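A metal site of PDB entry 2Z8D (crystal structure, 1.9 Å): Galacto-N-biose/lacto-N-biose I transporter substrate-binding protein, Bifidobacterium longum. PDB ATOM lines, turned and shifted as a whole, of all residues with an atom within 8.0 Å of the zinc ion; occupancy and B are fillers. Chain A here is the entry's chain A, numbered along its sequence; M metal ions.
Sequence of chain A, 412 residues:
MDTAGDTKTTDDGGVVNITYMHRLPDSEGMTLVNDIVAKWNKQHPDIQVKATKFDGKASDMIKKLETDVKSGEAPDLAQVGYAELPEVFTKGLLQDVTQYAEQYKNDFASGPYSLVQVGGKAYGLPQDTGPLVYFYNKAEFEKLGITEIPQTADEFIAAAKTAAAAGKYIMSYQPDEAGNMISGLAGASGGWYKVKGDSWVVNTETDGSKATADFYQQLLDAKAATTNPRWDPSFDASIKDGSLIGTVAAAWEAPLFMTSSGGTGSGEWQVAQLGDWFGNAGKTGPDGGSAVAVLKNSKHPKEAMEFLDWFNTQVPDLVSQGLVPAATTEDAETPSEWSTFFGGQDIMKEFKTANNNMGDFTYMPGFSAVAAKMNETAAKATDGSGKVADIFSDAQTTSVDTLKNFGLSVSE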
ATOM      1  N   ASP A  11     -20.540 -15.783   6.942  1.00  0.00           N
ATOM      2  CA  ASP A  11     -21.297 -16.436   8.057  1.00  0.00           C
ATOM      3  C   ASP A  11     -20.543 -16.398   9.369  1.00  0.00           C
ATOM      4  O   ASP A  11     -19.284 -16.380   9.404  1.00  0.00           O
ATOM      5  CB  ASP A  11     -21.655 -17.910   7.713  1.00  0.00           C
ATOM      6  CG  ASP A  11     -23.062 -18.059   7.115  1.00  0.00           C
ATOM      7  OD1 ASP A  11     -23.772 -17.053   6.865  1.00  0.00           O
ATOM      8  OD2 ASP A  11     -23.475 -19.187   6.816  1.00  0.00           O
ATOM      9  N   ASP A  12     -21.292 -16.406  10.470  1.00  0.00           N
ATOM     10  CA  ASP A  12     -20.718 -16.547  11.810  1.00  0.00           C
ATOM     11  C   ASP A  12     -19.879 -17.816  11.954  1.00  0.00           C
ATOM     12  O   ASP A  12     -19.987 -18.732  11.153  1.00  0.00           O
ATOM     13  CB  ASP A  12     -21.848 -16.567  12.837  1.00  0.00           C
ATOM     14  CG  ASP A  12     -22.543 -15.226  12.982  1.00  0.00           C
ATOM     15  OD1 ASP A  12     -21.897 -14.181  12.667  1.00  0.00           O
ATOM     16  OD2 ASP A  12     -23.719 -15.198  13.406  1.00  0.00           O
ATOM     17  N   GLY A  13     -19.092 -17.893  13.023  1.00  0.00           N
ATOM     18  CA  GLY A  13     -18.396 -19.139  13.387  1.00  0.00           C
ATOM     19  C   GLY A  13     -19.440 -20.179  13.777  1.00  0.00           C
ATOM     20  O   GLY A  13     -20.642 -19.878  13.929  1.00  0.00           O
ATOM     21  N   VAL A  16     -21.964 -19.338  18.238  1.00  0.00           N
ATOM     22  CA  VAL A  16     -22.165 -17.975  18.664  1.00  0.00           C
ATOM     23  C   VAL A  16     -22.567 -18.035  20.143  1.00  0.00           C
ATOM     24  O   VAL A  16     -23.337 -18.911  20.516  1.00  0.00           O
ATOM     25  CB  VAL A  16     -23.270 -17.293  17.817  1.00  0.00           C
ATOM     26  CG1 VAL A  16     -23.813 -16.071  18.517  1.00  0.00           C
ATOM     27  CG2 VAL A  16     -22.691 -16.966  16.412  1.00  0.00           C
ATOM     28  N   ASN A  17     -22.053 -17.099  20.948  1.00  0.00           N
ATOM     29  CA  ASN A  17     -22.370 -17.015  22.375  1.00  0.00           C
ATOM     30  C   ASN A  17     -23.096 -15.699  22.689  1.00  0.00           C
ATOM     31  O   ASN A  17     -22.548 -14.609  22.464  1.00  0.00           O
ATOM     32  CB  ASN A  17     -21.100 -17.122  23.233  1.00  0.00           C
ATOM     33  CG  ASN A  17     -20.464 -18.504  23.174  1.00  0.00           C
ATOM     34  OD1 ASN A  17     -20.943 -19.448  23.819  1.00  0.00           O
ATOM     35  ND2 ASN A  17     -19.348 -18.615  22.449  1.00  0.00           N
ATOM     36  N   ILE A  18     -24.292 -15.855  23.235  1.00  0.00           N
ATOM     37  CA  ILE A  18     -25.249 -14.815  23.547  1.00  0.00           C
ATOM     38  C   ILE A  18     -25.380 -14.749  25.076  1.00  0.00           C
ATOM     39  O   ILE A  18     -25.436 -15.780  25.710  1.00  0.00           O
ATOM     40  CB  ILE A  18     -26.618 -15.196  22.907  1.00  0.00           C
ATOM     41  CG1 ILE A  18     -26.531 -15.143  21.386  1.00  0.00           C
ATOM     42  CG2 ILE A  18     -27.763 -14.310  23.394  1.00  0.00           C
ATOM     43  CD1 ILE A  18     -25.772 -13.945  20.858  1.00  0.00           C
ATOM     44  N   ASP A  46     -25.105 -24.340  18.081  1.00  0.00           N
ATOM     45  CA  ASP A  46     -24.706 -23.205  17.257  1.00  0.00           C
ATOM     46  C   ASP A  46     -24.918 -21.779  17.877  1.00  0.00           C
ATOM     47  O   ASP A  46     -24.258 -20.789  17.480  1.00  0.00           O
ATOM     48  CB  ASP A  46     -25.356 -23.330  15.863  1.00  0.00           C
ATOM     49  CG  ASP A  46     -26.866 -23.247  15.894  1.00  0.00           C
ATOM     50  OD1 ASP A  46     -27.527 -24.098  16.556  1.00  0.00           O
ATOM     51  OD2 ASP A  46     -27.427 -22.387  15.170  1.00  0.00           O
ATOM     52  N   ILE A  47     -25.832 -21.689  18.850  1.00  0.00           N
ATOM     53  CA  ILE A  47     -26.142 -20.463  19.563  1.00  0.00           C
ATOM     54  C   ILE A  47     -26.341 -20.735  21.052  1.00  0.00           C
ATOM     55  O   ILE A  47     -27.440 -21.082  21.470  1.00  0.00           O
ATOM     56  CB  ILE A  47     -27.463 -19.811  19.073  1.00  0.00           C
ATOM     57  CG1 ILE A  47     -27.413 -19.554  17.559  1.00  0.00           C
ATOM     58  CG2 ILE A  47     -27.736 -18.522  19.887  1.00  0.00           C
ATOM     59  CD1 ILE A  47     -28.816 -19.259  16.920  1.00  0.00           C
ATOM     60  N   TYR A 100     -34.915  -7.928  12.035  1.00  0.00           N
ATOM     61  CA  TYR A 100     -35.108  -9.215  12.674  1.00  0.00           C
ATOM     62  C   TYR A 100     -36.478  -9.320  13.326  1.00  0.00           C
ATOM     63  O   TYR A 100     -37.198 -10.282  13.143  1.00  0.00           O
ATOM     64  CB  TYR A 100     -33.973  -9.466  13.660  1.00  0.00           C
ATOM     65  CG  TYR A 100     -32.613  -9.298  13.029  1.00  0.00           C
ATOM     66  CD1 TYR A 100     -32.183 -10.139  12.010  1.00  0.00           C
ATOM     67  CD2 TYR A 100     -31.748  -8.300  13.480  1.00  0.00           C
ATOM     68  CE1 TYR A 100     -30.921  -9.986  11.425  1.00  0.00           C
ATOM     69  CE2 TYR A 100     -30.469  -8.148  12.910  1.00  0.00           C
ATOM     70  CZ  TYR A 100     -30.079  -8.995  11.882  1.00  0.00           C
ATOM     71  OH  TYR A 100     -28.819  -8.834  11.351  1.00  0.00           O
ATOM     72  N   SER A 298     -23.962  -5.429  20.809  1.00  0.00           N
ATOM     73  CA  SER A 298     -24.065  -6.870  20.479  1.00  0.00           C
ATOM     74  C   SER A 298     -23.638  -7.127  19.033  1.00  0.00           C
ATOM     75  O   SER A 298     -24.103  -6.467  18.110  1.00  0.00           O
ATOM     76  CB  SER A 298     -25.484  -7.417  20.732  1.00  0.00           C
ATOM     77  OG  SER A 298     -25.598  -8.779  20.292  1.00  0.00           O
ATOM     78  N   LYS A 299     -22.702  -8.071  18.862  1.00  0.00           N
ATOM     79  CA  LYS A 299     -22.199  -8.491  17.545  1.00  0.00           C
ATOM     80  C   LYS A 299     -23.142  -9.474  16.844  1.00  0.00           C
ATOM     81  O   LYS A 299     -23.017  -9.720  15.612  1.00  0.00           O
ATOM     82  CB  LYS A 299     -20.794  -9.138  17.679  1.00  0.00           C
ATOM     83  CG  LYS A 299     -19.737  -8.260  18.344  1.00  0.00           C
ATOM     84  CD  LYS A 299     -19.489  -6.942  17.572  1.00  0.00           C
ATOM     85  CE  LYS A 299     -18.213  -6.990  16.719  1.00  0.00           C
ATOM     86  NZ  LYS A 299     -18.407  -6.276  15.425  1.00  0.00           N
ATOM     87  N   HIS A 300     -24.100 -10.039  17.595  1.00  0.00           N
ATOM     88  CA  HIS A 300     -24.990 -11.059  17.050  1.00  0.00           C
ATOM     89  C   HIS A 300     -26.470 -10.768  17.228  1.00  0.00           C
ATOM     90  O   HIS A 300     -27.205 -11.589  17.780  1.00  0.00           O
ATOM     91  CB  HIS A 300     -24.612 -12.446  17.587  1.00  0.00           C
ATOM     92  CG  HIS A 300     -23.201 -12.824  17.247  1.00  0.00           C
ATOM     93  ND1 HIS A 300     -22.830 -13.299  16.004  1.00  0.00           N
ATOM     94  CD2 HIS A 300     -22.056 -12.718  17.959  1.00  0.00           C
ATOM     95  CE1 HIS A 300     -21.536 -13.514  15.981  1.00  0.00           C
ATOM     96  NE2 HIS A 300     -21.033 -13.175  17.158  1.00  0.00           N
ATOM     97  N   PRO A 301     -26.928  -9.633  16.677  1.00  0.00           N
ATOM     98  CA  PRO A 301     -28.368  -9.315  16.803  1.00  0.00           C
ATOM     99  C   PRO A 301     -29.267 -10.382  16.198  1.00  0.00           C
ATOM    100  O   PRO A 301     -30.351 -10.629  16.749  1.00  0.00           O
ATOM    101  CB  PRO A 301     -28.522  -7.992  16.024  1.00  0.00           C
ATOM    102  CG  PRO A 301     -27.303  -7.946  15.107  1.00  0.00           C
ATOM    103  CD  PRO A 301     -26.207  -8.601  15.913  1.00  0.00           C
ATOM    104  N   LYS A 302     -28.904 -10.970  15.053  1.00  0.00           N
ATOM    105  CA  LYS A 302     -29.792 -11.982  14.472  1.00  0.00           C
ATOM    106  C   LYS A 302     -30.076 -13.164  15.409  1.00  0.00           C
ATOM    107  O   LYS A 302     -31.207 -13.558  15.654  1.00  0.00           O
ATOM    108  CB  LYS A 302     -29.324 -12.479  13.079  1.00  0.00           C
ATOM    109  CG  LYS A 302     -30.361 -13.410  12.472  1.00  0.00           C
ATOM    110  CD  LYS A 302     -30.260 -13.544  10.953  1.00  0.00           C
ATOM    111  CE  LYS A 302     -31.260 -14.590  10.482  1.00  0.00           C
ATOM    112  NZ  LYS A 302     -31.121 -15.009   9.056  1.00  0.00           N
ATOM    113  N   GLU A 303     -29.012 -13.753  15.910  1.00  0.00           N
ATOM    114  CA  GLU A 303     -29.165 -14.932  16.759  1.00  0.00           C
ATOM    115  C   GLU A 303     -29.690 -14.571  18.149  1.00  0.00           C
ATOM    116  O   GLU A 303     -30.388 -15.360  18.768  1.00  0.00           O
ATOM    117  CB  GLU A 303     -27.815 -15.685  16.858  1.00  0.00           C
ATOM    118  CG  GLU A 303     -27.334 -16.222  15.506  1.00  0.00           C
ATOM    119  CD  GLU A 303     -26.690 -15.175  14.640  1.00  0.00           C
ATOM    120  OE1 GLU A 303     -25.925 -14.370  15.197  1.00  0.00           O
ATOM    121  OE2 GLU A 303     -26.902 -15.139  13.382  1.00  0.00           O
ATOM    122  N   ALA A 304     -29.351 -13.392  18.640  1.00  0.00           N
ATOM    123  CA  ALA A 304     -29.970 -12.955  19.874  1.00  0.00           C
ATOM    124  C   ALA A 304     -31.504 -12.900  19.717  1.00  0.00           C
ATOM    125  O   ALA A 304     -32.276 -13.306  20.601  1.00  0.00           O
ATOM    126  CB  ALA A 304     -29.391 -11.570  20.316  1.00  0.00           C
HETATM  127 ZN    ZN M   1     -24.271 -13.566  14.473  1.00  0.00          ZN
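The backbone NH (N) of His 300 sits close to the side-chain hydroxyl (OG) of Ser 298, 3.3 Å away.
Of the 16 residues printed, 3 come within 4 Å of the zinc ion.
The zinc ion is bound by OE1 of Glu 303 (2.0 Å), OD2 of Asp 12 (2.0 Å) and ND1 of His 300 (2.1 Å).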
